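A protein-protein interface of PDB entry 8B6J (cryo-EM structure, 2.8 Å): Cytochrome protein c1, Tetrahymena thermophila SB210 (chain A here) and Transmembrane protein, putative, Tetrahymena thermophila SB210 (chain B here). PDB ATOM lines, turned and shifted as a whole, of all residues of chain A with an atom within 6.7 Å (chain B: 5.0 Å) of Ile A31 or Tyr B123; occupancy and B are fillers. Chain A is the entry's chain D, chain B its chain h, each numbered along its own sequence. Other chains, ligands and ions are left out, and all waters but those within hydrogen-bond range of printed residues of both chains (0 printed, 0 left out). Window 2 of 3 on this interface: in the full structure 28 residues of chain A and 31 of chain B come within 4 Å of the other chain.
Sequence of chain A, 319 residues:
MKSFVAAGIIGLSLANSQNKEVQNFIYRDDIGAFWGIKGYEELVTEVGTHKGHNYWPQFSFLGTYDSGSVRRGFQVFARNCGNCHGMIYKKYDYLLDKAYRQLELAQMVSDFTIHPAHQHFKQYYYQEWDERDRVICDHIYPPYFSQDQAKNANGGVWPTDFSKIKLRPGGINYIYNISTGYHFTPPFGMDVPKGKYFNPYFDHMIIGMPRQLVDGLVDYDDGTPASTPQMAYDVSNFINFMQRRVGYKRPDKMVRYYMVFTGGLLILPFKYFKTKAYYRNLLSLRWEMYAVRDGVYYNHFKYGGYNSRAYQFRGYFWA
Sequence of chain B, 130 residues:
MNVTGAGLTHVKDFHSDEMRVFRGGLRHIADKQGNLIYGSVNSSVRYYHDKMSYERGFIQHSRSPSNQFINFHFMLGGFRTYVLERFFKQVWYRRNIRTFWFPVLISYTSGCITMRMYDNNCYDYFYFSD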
ATOM      1  N   TYR A  27      20.229  11.702 -31.696  1.00  0.00           N
ATOM      2  CA  TYR A  27      19.053  11.549 -30.851  1.00  0.00           C
ATOM      3  C   TYR A  27      18.648  12.903 -30.290  1.00  0.00           C
ATOM      4  O   TYR A  27      19.461  13.591 -29.664  1.00  0.00           O
ATOM      5  CB  TYR A  27      19.337  10.554 -29.726  1.00  0.00           C
ATOM      6  CG  TYR A  27      20.048   9.320 -30.225  1.00  0.00           C
ATOM      7  CD1 TYR A  27      19.343   8.277 -30.809  1.00  0.00           C
ATOM      8  CD2 TYR A  27      21.426   9.207 -30.133  1.00  0.00           C
ATOM      9  CE1 TYR A  27      19.990   7.153 -31.276  1.00  0.00           C
ATOM     10  CE2 TYR A  27      22.082   8.087 -30.597  1.00  0.00           C
ATOM     11  CZ  TYR A  27      21.360   7.064 -31.169  1.00  0.00           C
ATOM     12  OH  TYR A  27      22.013   5.947 -31.632  1.00  0.00           O
ATOM     13  N   ARG A  28      17.393  13.278 -30.520  1.00  0.00           N
ATOM     14  CA  ARG A  28      16.907  14.580 -30.088  1.00  0.00           C
ATOM     15  C   ARG A  28      16.949  14.690 -28.569  1.00  0.00           C
ATOM     16  O   ARG A  28      16.654  13.732 -27.850  1.00  0.00           O
ATOM     17  CB  ARG A  28      15.486  14.798 -30.608  1.00  0.00           C
ATOM     18  CG  ARG A  28      14.844  16.081 -30.137  1.00  0.00           C
ATOM     19  CD  ARG A  28      13.618  16.425 -30.961  1.00  0.00           C
ATOM     20  NE  ARG A  28      13.969  16.917 -32.288  1.00  0.00           N
ATOM     21  CZ  ARG A  28      14.335  18.165 -32.552  1.00  0.00           C
ATOM     22  NH1 ARG A  28      14.435  19.074 -31.597  1.00  0.00           N
ATOM     23  NH2 ARG A  28      14.607  18.509 -33.807  1.00  0.00           N
ATOM     24  N   ASP A  29      17.323  15.871 -28.083  1.00  0.00           N
ATOM     25  CA  ASP A  29      17.606  16.085 -26.670  1.00  0.00           C
ATOM     26  C   ASP A  29      16.408  16.594 -25.878  1.00  0.00           C
ATOM     27  O   ASP A  29      16.525  16.778 -24.662  1.00  0.00           O
ATOM     28  CB  ASP A  29      18.770  17.071 -26.521  1.00  0.00           C
ATOM     29  CG  ASP A  29      19.545  16.872 -25.235  1.00  0.00           C
ATOM     30  OD1 ASP A  29      19.003  16.249 -24.298  1.00  0.00           O
ATOM     31  OD2 ASP A  29      20.701  17.341 -25.159  1.00  0.00           O
ATOM     32  N   ASP A  30      15.265  16.828 -26.522  1.00  0.00           N
ATOM     33  CA  ASP A  30      14.069  17.300 -25.835  1.00  0.00           C
ATOM     34  C   ASP A  30      12.937  16.283 -25.841  1.00  0.00           C
ATOM     35  O   ASP A  30      11.848  16.585 -25.343  1.00  0.00           O
ATOM     36  CB  ASP A  30      13.580  18.616 -26.455  1.00  0.00           C
ATOM     37  CG  ASP A  30      13.701  18.632 -27.964  1.00  0.00           C
ATOM     38  OD1 ASP A  30      14.812  18.377 -28.470  1.00  0.00           O
ATOM     39  OD2 ASP A  30      12.687  18.897 -28.643  1.00  0.00           O
ATOM     40  N   ILE A  31      13.161  15.087 -26.391  1.00  0.00           N
ATOM     41  CA  ILE A  31      12.129  14.056 -26.376  1.00  0.00           C
ATOM     42  C   ILE A  31      11.863  13.580 -24.958  1.00  0.00           C
ATOM     43  O   ILE A  31      10.750  13.144 -24.640  1.00  0.00           O
ATOM     44  CB  ILE A  31      12.539  12.882 -27.283  1.00  0.00           C
ATOM     45  CG1 ILE A  31      12.719  13.351 -28.726  1.00  0.00           C
ATOM     46  CG2 ILE A  31      11.513  11.767 -27.205  1.00  0.00           C
ATOM     47  CD1 ILE A  31      11.455  13.863 -29.370  1.00  0.00           C
ATOM     48  N   GLY A  32      12.864  13.651 -24.087  1.00  0.00           N
ATOM     49  CA  GLY A  32      12.798  13.047 -22.775  1.00  0.00           C
ATOM     50  C   GLY A  32      13.566  11.753 -22.652  1.00  0.00           C
ATOM     51  O   GLY A  32      13.532  11.132 -21.583  1.00  0.00           O
ATOM     52  N   ALA A  33      14.255  11.330 -23.707  1.00  0.00           N
ATOM     53  CA  ALA A  33      15.090  10.138 -23.698  1.00  0.00           C
ATOM     54  C   ALA A  33      16.543  10.568 -23.838  1.00  0.00           C
ATOM     55  O   ALA A  33      16.901  11.247 -24.804  1.00  0.00           O
ATOM     56  CB  ALA A  33      14.697   9.189 -24.830  1.00  0.00           C
ATOM     57  N   LYS A  38      15.006   5.172 -24.885  1.00  0.00           N
ATOM     58  CA  LYS A  38      13.585   5.433 -24.732  1.00  0.00           C
ATOM     59  C   LYS A  38      13.072   4.830 -23.429  1.00  0.00           C
ATOM     60  O   LYS A  38      13.719   3.990 -22.799  1.00  0.00           O
ATOM     61  CB  LYS A  38      12.806   4.874 -25.921  1.00  0.00           C
ATOM     62  CG  LYS A  38      13.066   5.605 -27.230  1.00  0.00           C
ATOM     63  CD  LYS A  38      12.556   7.036 -27.181  1.00  0.00           C
ATOM     64  CE  LYS A  38      12.682   7.719 -28.531  1.00  0.00           C
ATOM     65  NZ  LYS A  38      14.096   7.802 -28.982  1.00  0.00           N
ATOM     66  N   GLU A  41      10.220   8.495 -19.764  1.00  0.00           N
ATOM     67  CA  GLU A  41       9.805   9.784 -20.299  1.00  0.00           C
ATOM     68  C   GLU A  41       8.779  10.486 -19.422  1.00  0.00           C
ATOM     69  O   GLU A  41       8.398  11.620 -19.727  1.00  0.00           O
ATOM     70  CB  GLU A  41       9.249   9.601 -21.712  1.00  0.00           C
ATOM     71  CG  GLU A  41      10.319   9.215 -22.724  1.00  0.00           C
ATOM     72  CD  GLU A  41       9.830   8.240 -23.773  1.00  0.00           C
ATOM     73  OE1 GLU A  41       8.794   7.581 -23.550  1.00  0.00           O
ATOM     74  OE2 GLU A  41      10.490   8.128 -24.828  1.00  0.00           O
ATOM     75  N   GLU A  46      17.600  13.563 -16.107  1.00  0.00           N
ATOM     76  CA  GLU A  46      18.838  14.199 -16.533  1.00  0.00           C
ATOM     77  C   GLU A  46      19.431  15.123 -15.478  1.00  0.00           C
ATOM     78  O   GLU A  46      20.541  15.625 -15.674  1.00  0.00           O
ATOM     79  CB  GLU A  46      18.594  14.988 -17.823  1.00  0.00           C
ATOM     80  CG  GLU A  46      18.131  14.128 -18.989  1.00  0.00           C
ATOM     81  CD  GLU A  46      17.660  14.949 -20.173  1.00  0.00           C
ATOM     82  OE1 GLU A  46      17.700  16.194 -20.089  1.00  0.00           O
ATOM     83  OE2 GLU A  46      17.247  14.349 -21.187  1.00  0.00           O
ATOM     84  N   ASP B 119      12.471  10.923 -34.364  1.00  0.00           N
ATOM     85  CA  ASP B 119      12.393  11.687 -33.123  1.00  0.00           C
ATOM     86  C   ASP B 119      11.378  12.816 -33.227  1.00  0.00           C
ATOM     87  O   ASP B 119      10.700  13.136 -32.248  1.00  0.00           O
ATOM     88  CB  ASP B 119      13.769  12.242 -32.761  1.00  0.00           C
ATOM     89  CG  ASP B 119      14.739  11.161 -32.345  1.00  0.00           C
ATOM     90  OD1 ASP B 119      14.336   9.980 -32.314  1.00  0.00           O
ATOM     91  OD2 ASP B 119      15.905  11.492 -32.048  1.00  0.00           O
ATOM     92  N   ASN B 120      11.269  13.448 -34.396  1.00  0.00           N
ATOM     93  CA  ASN B 120      10.274  14.500 -34.568  1.00  0.00           C
ATOM     94  C   ASN B 120       8.860  13.938 -34.487  1.00  0.00           C
ATOM     95  O   ASN B 120       7.969  14.562 -33.899  1.00  0.00           O
ATOM     96  CB  ASN B 120      10.494  15.219 -35.896  1.00  0.00           C
ATOM     97  CG  ASN B 120      11.809  15.970 -35.939  1.00  0.00           C
ATOM     98  OD1 ASN B 120      12.373  16.314 -34.901  1.00  0.00           O
ATOM     99  ND2 ASN B 120      12.303  16.231 -37.142  1.00  0.00           N
ATOM    100  N   ASN B 121       8.634  12.758 -35.070  1.00  0.00           N
ATOM    101  CA  ASN B 121       7.334  12.112 -34.915  1.00  0.00           C
ATOM    102  C   ASN B 121       7.065  11.778 -33.453  1.00  0.00           C
ATOM    103  O   ASN B 121       5.941  11.946 -32.963  1.00  0.00           O
ATOM    104  CB  ASN B 121       7.263  10.851 -35.773  1.00  0.00           C
ATOM    105  CG  ASN B 121       7.188  11.157 -37.252  1.00  0.00           C
ATOM    106  OD1 ASN B 121       6.595  12.155 -37.662  1.00  0.00           O
ATOM    107  ND2 ASN B 121       7.790  10.298 -38.065  1.00  0.00           N
ATOM    108  N   CYS B 122       8.088  11.304 -32.740  1.00  0.00           N
ATOM    109  CA  CYS B 122       7.931  11.029 -31.314  1.00  0.00           C
ATOM    110  C   CYS B 122       7.574  12.296 -30.546  1.00  0.00           C
ATOM    111  O   CYS B 122       6.730  12.269 -29.642  1.00  0.00           O
ATOM    112  CB  CYS B 122       9.214  10.410 -30.763  1.00  0.00           C
ATOM    113  SG  CYS B 122       9.216  10.179 -28.979  1.00  0.00           S
ATOM    114  N   TYR B 123       8.219  13.413 -30.884  1.00  0.00           N
ATOM    115  CA  TYR B 123       7.905  14.688 -30.247  1.00  0.00           C
ATOM    116  C   TYR B 123       6.459  15.083 -30.510  1.00  0.00           C
ATOM    117  O   TYR B 123       5.734  15.481 -29.592  1.00  0.00           O
ATOM    118  CB  TYR B 123       8.857  15.769 -30.759  1.00  0.00           C
ATOM    119  CG  TYR B 123       8.681  17.117 -30.101  1.00  0.00           C
ATOM    120  CD1 TYR B 123       7.738  18.021 -30.567  1.00  0.00           C
ATOM    121  CD2 TYR B 123       9.466  17.489 -29.020  1.00  0.00           C
ATOM    122  CE1 TYR B 123       7.576  19.253 -29.969  1.00  0.00           C
ATOM    123  CE2 TYR B 123       9.312  18.721 -28.416  1.00  0.00           C
ATOM    124  CZ  TYR B 123       8.366  19.598 -28.895  1.00  0.00           C
ATOM    125  OH  TYR B 123       8.209  20.827 -28.296  1.00  0.00           O
ATOM    126  N   ASP B 124       6.022  14.976 -31.766  1.00  0.00           N
ATOM    127  CA  ASP B 124       4.636  15.298 -32.089  1.00  0.00           C
ATOM    128  C   ASP B 124       3.678  14.425 -31.292  1.00  0.00           C
ATOM    129  O   ASP B 124       2.621  14.890 -30.850  1.00  0.00           O
ATOM    130  CB  ASP B 124       4.388  15.133 -33.587  1.00  0.00           C
ATOM    131  CG  ASP B 124       5.115  16.171 -34.415  1.00  0.00           C
ATOM    132  OD1 ASP B 124       5.852  16.993 -33.828  1.00  0.00           O
ATOM    133  OD2 ASP B 124       4.947  16.171 -35.652  1.00  0.00           O
ATOM    134  N   TYR B 125       4.027  13.152 -31.106  1.00  0.00           N
ATOM    135  CA  TYR B 125       3.196  12.273 -30.290  1.00  0.00           C
ATOM    136  C   TYR B 125       3.136  12.760 -28.847  1.00  0.00           C
ATOM    137  O   TYR B 125       2.053  12.871 -28.261  1.00  0.00           O
ATOM    138  CB  TYR B 125       3.735  10.844 -30.352  1.00  0.00           C
ATOM    139  CG  TYR B 125       3.087   9.900 -29.365  1.00  0.00           C
ATOM    140  CD1 TYR B 125       1.931   9.211 -29.692  1.00  0.00           C
ATOM    141  CD2 TYR B 125       3.637   9.696 -28.108  1.00  0.00           C
ATOM    142  CE1 TYR B 125       1.337   8.346 -28.794  1.00  0.00           C
ATOM    143  CE2 TYR B 125       3.052   8.836 -27.203  1.00  0.00           C
ATOM    144  CZ  TYR B 125       1.902   8.164 -27.551  1.00  0.00           C
ATOM    145  OH  TYR B 125       1.316   7.305 -26.652  1.00  0.00           O
ATOM    146  N   PHE B 126       4.295  13.058 -28.256  1.00  0.00           N
ATOM    147  CA  PHE B 126       4.326  13.432 -26.845  1.00  0.00           C
ATOM    148  C   PHE B 126       3.801  14.844 -26.623  1.00  0.00           C
ATOM    149  O   PHE B 126       3.044  15.088 -25.678  1.00  0.00           O
ATOM    150  CB  PHE B 126       5.746  13.308 -26.295  1.00  0.00           C
ATOM    151  CG  PHE B 126       6.107  11.921 -25.853  1.00  0.00           C
ATOM    152  CD1 PHE B 126       5.475  11.343 -24.770  1.00  0.00           C
ATOM    153  CD2 PHE B 126       7.087  11.202 -26.511  1.00  0.00           C
ATOM    154  CE1 PHE B 126       5.804  10.071 -24.356  1.00  0.00           C
ATOM    155  CE2 PHE B 126       7.419   9.929 -26.099  1.00  0.00           C
ATOM    156  CZ  PHE B 126       6.777   9.364 -25.021  1.00  0.00           C
ATOM    157  N   TYR B 127       4.190  15.785 -27.476  1.00  0.00           N
ATOM    158  CA  TYR B 127       3.898  17.198 -27.277  1.00  0.00           C
ATOM    159  C   TYR B 127       2.811  17.652 -28.238  1.00  0.00           C
ATOM    160  O   TYR B 127       2.906  17.423 -29.447  1.00  0.00           O
ATOM    161  CB  TYR B 127       5.152  18.050 -27.478  1.00  0.00           C
ATOM    162  CG  TYR B 127       6.197  17.875 -26.402  1.00  0.00           C
ATOM    163  CD1 TYR B 127       7.188  16.912 -26.519  1.00  0.00           C
ATOM    164  CD2 TYR B 127       6.196  18.678 -25.273  1.00  0.00           C
ATOM    165  CE1 TYR B 127       8.145  16.751 -25.541  1.00  0.00           C
ATOM    166  CE2 TYR B 127       7.149  18.524 -24.289  1.00  0.00           C
ATOM    167  CZ  TYR B 127       8.122  17.560 -24.429  1.00  0.00           C
ATOM    168  OH  TYR B 127       9.075  17.405 -23.449  1.00  0.00           O
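NH1 of Arg A28 lies within salt-bridge range of OD1 of Asp A30 (3.2 Å).
Among the printed residues, merely in contact across the chains: Tyr A27 with Asp B119, Asp A30 with Tyr B123, Ile A31 with Asp B119, Ile A31 with Cys B122, Ile A31 with Tyr B123 and Glu A41 with Phe B126.
Hydrophobic or aromatic side chains of chain A within 4 Å of the printed part of chain B: Ile A31. Along chain A the printed residues that touch a printed residue of chain B span positions 27 to 41. Of the 9 printed residues of chain B, 6 touch a printed residue of chain A. Among the printed residues, 10 pairs touch across the chains. Among the printed residues, Asp or Glu carboxylates within 4 Å of a Lys or Arg side-chain nitrogen of the other chain: Lys A38 with Asp B119 (3.99 Å).
OD2 of Asp B119 is in hydrogen-bond range of N of Arg A28, 2.8 Å away. The side-chain amide oxygen of Asn B120 lies within hydrogen-bond range of the guanidinium group of Arg A28 (3.1 Å). The backbone carbonyl oxygen (O) of Asp A30 is in hydrogen-bond range of the side-chain hydroxyl (OH) of Tyr B127 (3.5 Å). NZ of Lys A38 is in salt-bridge range of OD1 of Asp B119 (3.99 Å).
Ile A31 touches just these residues of chain B: Asp B119 (3.1 Å), Cys B122 (3.3 Å) and Tyr B123 (3.5 Å). Of chain A, only Asp A30 (3.4 Å) and Ile A31 (3.5 Å) come within 4 Å of Tyr B123. Printed residues of chain B within 4 Å of Tyr A27: Asp B119. Printed residues of chain A within 4 Å of Tyr B127: Asp A30 (3.5 Å). Printed residues of chain A within 4 Å of Cys B122: Ile A31. Of the printed residues of chain A, Phe B126 touches Glu A41 (3.1 Å). Printed residues of chain A within 4 Å of Asp B119: Tyr A27, Arg A28, Ile A31 and Lys A38. Asp A29 touches none of the printed residues of chain B.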
